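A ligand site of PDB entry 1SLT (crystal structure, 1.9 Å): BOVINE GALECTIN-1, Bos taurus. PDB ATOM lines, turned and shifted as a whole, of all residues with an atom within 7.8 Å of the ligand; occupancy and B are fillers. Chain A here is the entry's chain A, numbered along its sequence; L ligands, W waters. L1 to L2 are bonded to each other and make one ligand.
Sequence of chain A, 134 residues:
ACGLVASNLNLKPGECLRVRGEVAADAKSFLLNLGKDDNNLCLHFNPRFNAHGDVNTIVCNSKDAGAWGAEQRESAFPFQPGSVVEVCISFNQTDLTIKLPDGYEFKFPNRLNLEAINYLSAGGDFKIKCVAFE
The side-chain carboxylate of Glu 71 lies within hydrogen-bond range of an oxygen (O2) of LIG L1 (2.4 Å). O5 of LG2 L2 is in hydrogen-bond range of ND2 of Asn 61 (2.7 Å). O2 of LIG L1 sits at hydrogen-bond distance from NH1 of Arg 48. O3 of LG2 L2 sits at hydrogen-bond distance from NE2 of His 44, 2.8 Å away. NH2 of Arg 73 lies within hydrogen-bond range of O2 of LIG L1 (3.3 Å). An oxygen (O3) of LG2 L2 sits at hydrogen-bond distance from the side-chain amide oxygen (OD1) of Asn 46 (3.4 Å).
Water W1 lies within hydrogen-bond range of O of His 52 (2.6 Å), N1 of LIG L1 (2.6 Å), OD2 of Asp 54 (2.8 Å) and NH2 of Arg 73 (3.2 Å). Water W3 lies within hydrogen-bond range of O2 of LG2 L2 (2.7 Å) and OD1 of Asn 46 (2.9 Å).
The backbone carbonyl oxygen (O) of Asn 61 lies within hydrogen-bond range of the backbone NH (N) of His 44 (2.8 Å). O of Gly 69 lies within hydrogen-bond range of ND2 of Asn 61 (3.0 Å). O of Ala 70 sits close to OD1 of Asn 61, at 3.2 Å. NH1 of Arg 48 lies within salt-bridge range of OD2 of Asp 54, 2.7 Å away. A ring nitrogen (ND1) of His 44 sits at hydrogen-bond distance from the side-chain amide oxygen (OD1) of Asn 33, at 2.8 Å. OD2 of Asp 54 is in salt-bridge range of NH2 of Arg 73, at 2.8 Å. The backbone NH (N) of Asn 46 sits at hydrogen-bond distance from the backbone carbonyl oxygen (O) of Val 59, 2.8 Å away. The side-chain amide nitrogen (ND2) of Asn 46 lies within hydrogen-bond range of the side-chain hydroxyl (OG) of Ser 29.
CE1 of His 52 touches O1 of LG2 L2 (3.97 Å). CZ2 of Trp 68 touches C4 of LG2 L2, at 3.5 Å. Of the 23 residues printed, 8 come within 4 Å of the ligand.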
ATOM      1  N   SER A  29     -14.883 -17.932  18.671  1.00  0.00           N
ATOM      2  CA  SER A  29     -15.422 -18.362  17.377  1.00  0.00           C
ATOM      3  C   SER A  29     -14.414 -19.242  16.664  1.00  0.00           C
ATOM      4  O   SER A  29     -13.210 -19.143  16.959  1.00  0.00           O
ATOM      5  CB  SER A  29     -15.363 -17.080  16.549  1.00  0.00           C
ATOM      6  OG  SER A  29     -15.764 -17.289  15.229  1.00  0.00           O
ATOM      7  N   LEU A  31     -13.797 -21.362  12.572  1.00  0.00           N
ATOM      8  CA  LEU A  31     -14.385 -21.558  11.288  1.00  0.00           C
ATOM      9  C   LEU A  31     -13.558 -22.631  10.558  1.00  0.00           C
ATOM     10  O   LEU A  31     -12.407 -22.857  10.942  1.00  0.00           O
ATOM     11  CB  LEU A  31     -14.313 -20.196  10.562  1.00  0.00           C
ATOM     12  CG  LEU A  31     -12.919 -19.755  10.265  1.00  0.00           C
ATOM     13  CD1 LEU A  31     -12.570 -20.349   8.911  1.00  0.00           C
ATOM     14  CD2 LEU A  31     -12.982 -18.286  10.077  1.00  0.00           C
ATOM     15  N   ASN A  33     -13.428 -23.418   6.337  1.00  0.00           N
ATOM     16  CA  ASN A  33     -13.696 -23.004   5.005  1.00  0.00           C
ATOM     17  C   ASN A  33     -13.398 -24.146   4.039  1.00  0.00           C
ATOM     18  O   ASN A  33     -12.308 -24.745   4.121  1.00  0.00           O
ATOM     19  CB  ASN A  33     -12.869 -21.821   4.583  1.00  0.00           C
ATOM     20  CG  ASN A  33     -13.401 -20.602   5.277  1.00  0.00           C
ATOM     21  OD1 ASN A  33     -14.563 -20.551   5.680  1.00  0.00           O
ATOM     22  ND2 ASN A  33     -12.574 -19.617   5.402  1.00  0.00           N
ATOM     23  N   HIS A  44     -18.575 -21.987   4.346  1.00  0.00           N
ATOM     24  CA  HIS A  44     -17.880 -21.288   5.440  1.00  0.00           C
ATOM     25  C   HIS A  44     -18.715 -21.735   6.719  1.00  0.00           C
ATOM     26  O   HIS A  44     -19.929 -21.429   6.843  1.00  0.00           O
ATOM     27  CB  HIS A  44     -17.885 -19.796   5.183  1.00  0.00           C
ATOM     28  CG  HIS A  44     -17.588 -18.928   6.389  1.00  0.00           C
ATOM     29  ND1 HIS A  44     -16.307 -18.762   6.861  1.00  0.00           N
ATOM     30  CD2 HIS A  44     -18.455 -18.149   7.165  1.00  0.00           C
ATOM     31  CE1 HIS A  44     -16.319 -17.919   7.885  1.00  0.00           C
ATOM     32  NE2 HIS A  44     -17.612 -17.537   8.102  1.00  0.00           N
ATOM     33  N   PHE A  45     -18.172 -22.570   7.608  1.00  0.00           N
ATOM     34  CA  PHE A  45     -18.861 -23.124   8.798  1.00  0.00           C
ATOM     35  C   PHE A  45     -18.233 -22.397   9.964  1.00  0.00           C
ATOM     36  O   PHE A  45     -17.040 -22.479  10.184  1.00  0.00           O
ATOM     37  CB  PHE A  45     -18.638 -24.610   8.755  1.00  0.00           C
ATOM     38  CG  PHE A  45     -18.992 -25.340  10.007  1.00  0.00           C
ATOM     39  CD1 PHE A  45     -20.302 -25.763  10.255  1.00  0.00           C
ATOM     40  CD2 PHE A  45     -17.984 -25.603  10.939  1.00  0.00           C
ATOM     41  CE1 PHE A  45     -20.564 -26.523  11.396  1.00  0.00           C
ATOM     42  CE2 PHE A  45     -18.216 -26.319  12.105  1.00  0.00           C
ATOM     43  CZ  PHE A  45     -19.518 -26.797  12.278  1.00  0.00           C
ATOM     44  N   ASN A  46     -19.034 -21.544  10.642  1.00  0.00           N
ATOM     45  CA  ASN A  46     -18.534 -20.753  11.703  1.00  0.00           C
ATOM     46  C   ASN A  46     -19.343 -20.753  13.019  1.00  0.00           C
ATOM     47  O   ASN A  46     -20.181 -19.853  13.162  1.00  0.00           O
ATOM     48  CB  ASN A  46     -18.640 -19.377  11.077  1.00  0.00           C
ATOM     49  CG  ASN A  46     -18.100 -18.304  11.992  1.00  0.00           C
ATOM     50  OD1 ASN A  46     -18.357 -17.140  11.730  1.00  0.00           O
ATOM     51  ND2 ASN A  46     -17.281 -18.675  13.013  1.00  0.00           N
ATOM     52  N   ARG A  48     -20.219 -19.681  16.434  1.00  0.00           N
ATOM     53  CA  ARG A  48     -19.843 -18.507  17.220  1.00  0.00           C
ATOM     54  C   ARG A  48     -20.252 -18.734  18.687  1.00  0.00           C
ATOM     55  O   ARG A  48     -21.453 -18.938  19.000  1.00  0.00           O
ATOM     56  CB  ARG A  48     -20.314 -17.154  16.664  1.00  0.00           C
ATOM     57  CG  ARG A  48     -20.239 -17.096  15.162  1.00  0.00           C
ATOM     58  CD  ARG A  48     -20.495 -15.708  14.641  1.00  0.00           C
ATOM     59  NE  ARG A  48     -20.236 -15.529  13.214  1.00  0.00           N
ATOM     60  CZ  ARG A  48     -20.902 -14.738  12.379  1.00  0.00           C
ATOM     61  NH1 ARG A  48     -21.947 -13.951  12.737  1.00  0.00           N
ATOM     62  NH2 ARG A  48     -20.509 -14.667  11.100  1.00  0.00           N
ATOM     63  N   ALA A  51     -19.619 -14.012  19.223  1.00  0.00           N
ATOM     64  CA  ALA A  51     -18.887 -13.087  18.368  1.00  0.00           C
ATOM     65  C   ALA A  51     -19.823 -12.459  17.342  1.00  0.00           C
ATOM     66  O   ALA A  51     -20.757 -13.187  17.009  1.00  0.00           O
ATOM     67  CB  ALA A  51     -17.719 -13.818  17.712  1.00  0.00           C
ATOM     68  N   HIS A  52     -19.619 -11.219  16.861  1.00  0.00           N
ATOM     69  CA  HIS A  52     -20.491 -10.568  15.849  1.00  0.00           C
ATOM     70  C   HIS A  52     -21.922 -10.505  16.327  1.00  0.00           C
ATOM     71  O   HIS A  52     -22.880 -10.538  15.559  1.00  0.00           O
ATOM     72  CB  HIS A  52     -20.578 -11.221  14.443  1.00  0.00           C
ATOM     73  CG  HIS A  52     -19.206 -11.623  14.109  1.00  0.00           C
ATOM     74  ND1 HIS A  52     -18.286 -10.652  13.787  1.00  0.00           N
ATOM     75  CD2 HIS A  52     -18.608 -12.839  14.166  1.00  0.00           C
ATOM     76  CE1 HIS A  52     -17.146 -11.295  13.643  1.00  0.00           C
ATOM     77  NE2 HIS A  52     -17.291 -12.604  13.855  1.00  0.00           N
ATOM     78  N   GLY A  53     -22.034 -10.469  17.618  1.00  0.00           N
ATOM     79  CA  GLY A  53     -23.333 -10.408  18.125  1.00  0.00           C
ATOM     80  C   GLY A  53     -23.965 -11.741  18.174  1.00  0.00           C
ATOM     81  O   GLY A  53     -25.136 -11.748  18.431  1.00  0.00           O
ATOM     82  N   ASP A  54     -23.312 -12.854  17.936  1.00  0.00           N
ATOM     83  CA  ASP A  54     -24.075 -14.067  17.977  1.00  0.00           C
ATOM     84  C   ASP A  54     -23.638 -14.820  19.208  1.00  0.00           C
ATOM     85  O   ASP A  54     -22.468 -14.609  19.609  1.00  0.00           O
ATOM     86  CB  ASP A  54     -23.882 -14.899  16.675  1.00  0.00           C
ATOM     87  CG  ASP A  54     -24.726 -14.501  15.474  1.00  0.00           C
ATOM     88  OD1 ASP A  54     -25.953 -14.597  15.380  1.00  0.00           O
ATOM     89  OD2 ASP A  54     -24.039 -14.019  14.480  1.00  0.00           O
ATOM     90  N   VAL A  59     -23.182 -20.153  12.221  1.00  0.00           N
ATOM     91  CA  VAL A  59     -23.501 -19.410  11.024  1.00  0.00           C
ATOM     92  C   VAL A  59     -22.771 -20.165   9.871  1.00  0.00           C
ATOM     93  O   VAL A  59     -21.551 -20.425   9.990  1.00  0.00           O
ATOM     94  CB  VAL A  59     -22.993 -17.938  11.087  1.00  0.00           C
ATOM     95  CG1 VAL A  59     -22.931 -17.115   9.782  1.00  0.00           C
ATOM     96  CG2 VAL A  59     -23.615 -17.173  12.245  1.00  0.00           C
ATOM     97  N   CYS A  60     -23.494 -20.472   8.787  1.00  0.00           N
ATOM     98  CA  CYS A  60     -22.998 -21.073   7.539  1.00  0.00           C
ATOM     99  C   CYS A  60     -23.243 -20.118   6.385  1.00  0.00           C
ATOM    100  O   CYS A  60     -24.262 -19.437   6.241  1.00  0.00           O
ATOM    101  CB  CYS A  60     -23.581 -22.409   7.167  1.00  0.00           C
ATOM    102  SG  CYS A  60     -23.270 -23.657   8.393  1.00  0.00           S
ATOM    103  N   ASN A  61     -22.253 -19.979   5.541  1.00  0.00           N
ATOM    104  CA  ASN A  61     -22.394 -19.133   4.387  1.00  0.00           C
ATOM    105  C   ASN A  61     -21.571 -19.749   3.215  1.00  0.00           C
ATOM    106  O   ASN A  61     -20.920 -20.788   3.351  1.00  0.00           O
ATOM    107  CB  ASN A  61     -21.983 -17.664   4.581  1.00  0.00           C
ATOM    108  CG  ASN A  61     -22.754 -16.700   3.676  1.00  0.00           C
ATOM    109  OD1 ASN A  61     -23.486 -17.064   2.714  1.00  0.00           O
ATOM    110  ND2 ASN A  61     -22.515 -15.452   4.049  1.00  0.00           N
ATOM    111  N   SER A  62     -21.668 -19.108   2.058  1.00  0.00           N
ATOM    112  CA  SER A  62     -20.948 -19.449   0.814  1.00  0.00           C
ATOM    113  C   SER A  62     -20.177 -18.136   0.544  1.00  0.00           C
ATOM    114  O   SER A  62     -20.372 -17.038   1.154  1.00  0.00           O
ATOM    115  CB  SER A  62     -21.791 -20.035  -0.342  1.00  0.00           C
ATOM    116  OG  SER A  62     -22.660 -18.983  -0.753  1.00  0.00           O
ATOM    117  N   LYS A  63     -19.193 -18.240  -0.340  1.00  0.00           N
ATOM    118  CA  LYS A  63     -18.420 -17.083  -0.741  1.00  0.00           C
ATOM    119  C   LYS A  63     -18.195 -17.314  -2.243  1.00  0.00           C
ATOM    120  O   LYS A  63     -17.781 -18.420  -2.670  1.00  0.00           O
ATOM    121  CB  LYS A  63     -17.212 -16.780   0.074  1.00  0.00           C
ATOM    122  CG  LYS A  63     -16.598 -15.521  -0.431  1.00  0.00           C
ATOM    123  CD  LYS A  63     -16.022 -14.858   0.771  1.00  0.00           C
ATOM    124  CE  LYS A  63     -14.536 -15.041   0.869  1.00  0.00           C
ATOM    125  NZ  LYS A  63     -14.095 -14.033   1.868  1.00  0.00           N
ATOM    126  N   TRP A  68     -19.485 -12.729   0.163  1.00  0.00           N
ATOM    127  CA  TRP A  68     -20.391 -13.620   0.913  1.00  0.00           C
ATOM    128  C   TRP A  68     -21.797 -13.731   0.382  1.00  0.00           C
ATOM    129  O   TRP A  68     -22.292 -12.780  -0.172  1.00  0.00           O
ATOM    130  CB  TRP A  68     -20.447 -13.072   2.302  1.00  0.00           C
ATOM    131  CG  TRP A  68     -19.157 -13.123   3.005  1.00  0.00           C
ATOM    132  CD1 TRP A  68     -18.442 -12.063   3.435  1.00  0.00           C
ATOM    133  CD2 TRP A  68     -18.514 -14.291   3.501  1.00  0.00           C
ATOM    134  NE1 TRP A  68     -17.393 -12.510   4.179  1.00  0.00           N
ATOM    135  CE2 TRP A  68     -17.387 -13.874   4.231  1.00  0.00           C
ATOM    136  CE3 TRP A  68     -18.850 -15.636   3.401  1.00  0.00           C
ATOM    137  CZ2 TRP A  68     -16.513 -14.725   4.894  1.00  0.00           C
ATOM    138  CZ3 TRP A  68     -18.025 -16.464   4.090  1.00  0.00           C
ATOM    139  CH2 TRP A  68     -16.882 -16.038   4.800  1.00  0.00           C
ATOM    140  N   GLY A  69     -22.460 -14.871   0.515  1.00  0.00           N
ATOM    141  CA  GLY A  69     -23.836 -15.146   0.112  1.00  0.00           C
ATOM    142  C   GLY A  69     -24.790 -14.866   1.352  1.00  0.00           C
ATOM    143  O   GLY A  69     -24.468 -14.073   2.251  1.00  0.00           O
ATOM    144  N   ALA A  70     -25.984 -15.474   1.367  1.00  0.00           N
ATOM    145  CA  ALA A  70     -26.999 -15.345   2.390  1.00  0.00           C
ATOM    146  C   ALA A  70     -26.674 -16.293   3.535  1.00  0.00           C
ATOM    147  O   ALA A  70     -26.566 -17.511   3.301  1.00  0.00           O
ATOM    148  CB  ALA A  70     -28.275 -15.835   1.739  1.00  0.00           C
ATOM    149  N   GLU A  71     -26.532 -15.747   4.767  1.00  0.00           N
ATOM    150  CA  GLU A  71     -26.255 -16.586   5.928  1.00  0.00           C
ATOM    151  C   GLU A  71     -27.352 -17.575   6.215  1.00  0.00           C
ATOM    152  O   GLU A  71     -28.520 -17.443   5.844  1.00  0.00           O
ATOM    153  CB  GLU A  71     -26.078 -15.736   7.174  1.00  0.00           C
ATOM    154  CG  GLU A  71     -24.889 -14.832   6.964  1.00  0.00           C
ATOM    155  CD  GLU A  71     -24.671 -14.176   8.266  1.00  0.00           C
ATOM    156  OE1 GLU A  71     -25.554 -14.235   9.116  1.00  0.00           O
ATOM    157  OE2 GLU A  71     -23.539 -13.490   8.310  1.00  0.00           O
ATOM    158  N   GLN A  72     -26.963 -18.613   6.914  1.00  0.00           N
ATOM    159  CA  GLN A  72     -27.887 -19.659   7.287  1.00  0.00           C
ATOM    160  C   GLN A  72     -27.458 -19.971   8.696  1.00  0.00           C
ATOM    161  O   GLN A  72     -26.278 -20.140   8.965  1.00  0.00           O
ATOM    162  CB  GLN A  72     -27.937 -20.773   6.263  1.00  0.00           C
ATOM    163  CG  GLN A  72     -28.437 -22.057   6.916  1.00  0.00           C
ATOM    164  CD  GLN A  72     -28.510 -23.181   5.888  1.00  0.00           C
ATOM    165  OE1 GLN A  72     -28.604 -22.818   4.712  1.00  0.00           O
ATOM    166  NE2 GLN A  72     -28.494 -24.467   6.344  1.00  0.00           N
ATOM    167  N   ARG A  73     -28.395 -19.904   9.651  1.00  0.00           N
ATOM    168  CA  ARG A  73     -28.047 -20.090  11.058  1.00  0.00           C
ATOM    169  C   ARG A  73     -28.641 -21.342  11.601  1.00  0.00           C
ATOM    170  O   ARG A  73     -29.719 -21.831  11.224  1.00  0.00           O
ATOM    171  CB  ARG A  73     -28.404 -18.900  11.930  1.00  0.00           C
ATOM    172  CG  ARG A  73     -27.614 -17.690  11.565  1.00  0.00           C
ATOM    173  CD  ARG A  73     -28.085 -16.420  12.264  1.00  0.00           C
ATOM    174  NE  ARG A  73     -27.025 -15.556  12.784  1.00  0.00           N
ATOM    175  CZ  ARG A  73     -26.505 -14.812  11.863  1.00  0.00           C
ATOM    176  NH1 ARG A  73     -27.061 -14.981  10.655  1.00  0.00           N
ATOM    177  NH2 ARG A  73     -25.506 -13.972  12.142  1.00  0.00           N
ATOM    178  N   ARG A 111     -24.107 -23.624  -3.383  1.00  0.00           N
ATOM    179  CA  ARG A 111     -24.510 -22.607  -4.284  1.00  0.00           C
ATOM    180  C   ARG A 111     -23.632 -22.300  -5.473  1.00  0.00           C
ATOM    181  O   ARG A 111     -24.062 -21.635  -6.449  1.00  0.00           O
ATOM    182  CB  ARG A 111     -24.717 -21.428  -3.353  1.00  0.00           C
ATOM    183  CG  ARG A 111     -25.649 -21.904  -2.231  1.00  0.00           C
ATOM    184  CD  ARG A 111     -26.509 -20.893  -1.516  1.00  0.00           C
ATOM    185  NE  ARG A 111     -25.745 -19.995  -0.665  1.00  0.00           N
ATOM    186  CZ  ARG A 111     -26.079 -19.361   0.479  1.00  0.00           C
ATOM    187  NH1 ARG A 111     -27.247 -19.492   1.069  1.00  0.00           N
ATOM    188  NH2 ARG A 111     -25.173 -18.555   1.060  1.00  0.00           N
HETATM  189  C1  LIG L   1     -23.983  -8.907  10.137  1.00  0.00           C
HETATM  190  C2  LIG L   1     -24.184 -10.444  10.324  1.00  0.00           C
HETATM  191  C3  LIG L   1     -22.832 -11.225  10.559  1.00  0.00           C
HETATM  192  C4  LIG L   1     -21.782 -10.784   9.526  1.00  0.00           C
HETATM  193  C5  LIG L   1     -21.713  -9.240   9.381  1.00  0.00           C
HETATM  194  C6  LIG L   1     -20.797  -8.687   8.287  1.00  0.00           C
HETATM  195  C7  LIG L   1     -26.592 -10.892  10.898  1.00  0.00           C
HETATM  196  C8  LIG L   1     -27.549 -11.369  11.971  1.00  0.00           C
HETATM  197  O1  LIG L   1     -23.019  -8.685   9.105  1.00  0.00           O
HETATM  198  O2  LIG L   1     -22.969 -12.660  10.534  1.00  0.00           O
HETATM  199  O3  LIG L   1     -20.487 -11.324   9.866  1.00  0.00           O
HETATM  200  O4  LIG L   1     -20.803  -9.395   7.030  1.00  0.00           O
HETATM  201  O5  LIG L   1     -27.032 -10.583   9.784  1.00  0.00           O
HETATM  202  N1  LIG L   1     -25.281 -10.838  11.222  1.00  0.00           N
HETATM  203  O6  LIG L   1     -23.341  -8.344  11.284  1.00  0.00           O
HETATM  204  C1  LG2 L   2     -19.742 -11.911   8.806  1.00  0.00           C
HETATM  205  C2  LG2 L   2     -18.366 -12.203   9.315  1.00  0.00           C
HETATM  206  C3  LG2 L   2     -17.520 -13.005   8.332  1.00  0.00           C
HETATM  207  C4  LG2 L   2     -18.274 -14.220   7.844  1.00  0.00           C
HETATM  208  C5  LG2 L   2     -19.682 -13.848   7.467  1.00  0.00           C
HETATM  209  C6  LG2 L   2     -20.582 -15.019   7.243  1.00  0.00           C
HETATM  210  O1  LG2 L   2     -17.722 -11.019   9.720  1.00  0.00           O
HETATM  211  O2  LG2 L   2     -16.454 -13.538   9.110  1.00  0.00           O
HETATM  212  O3  LG2 L   2     -18.394 -15.033   9.011  1.00  0.00           O
HETATM  213  O4  LG2 L   2     -20.258 -13.217   8.605  1.00  0.00           O
HETATM  214  O5  LG2 L   2     -21.700 -14.580   6.468  1.00  0.00           O
HETATM  215  O   HOH W   1     -24.480 -11.401  13.668  1.00  0.00           O
HETATM  216  O   HOH W   2     -16.997  -9.499   6.920  1.00  0.00           O
HETATM  217  O   HOH W   3     -16.361 -15.136  11.333  1.00  0.00           O
HETATM  218  O   HOH W   4     -14.262 -13.041   6.681  1.00  0.00           O
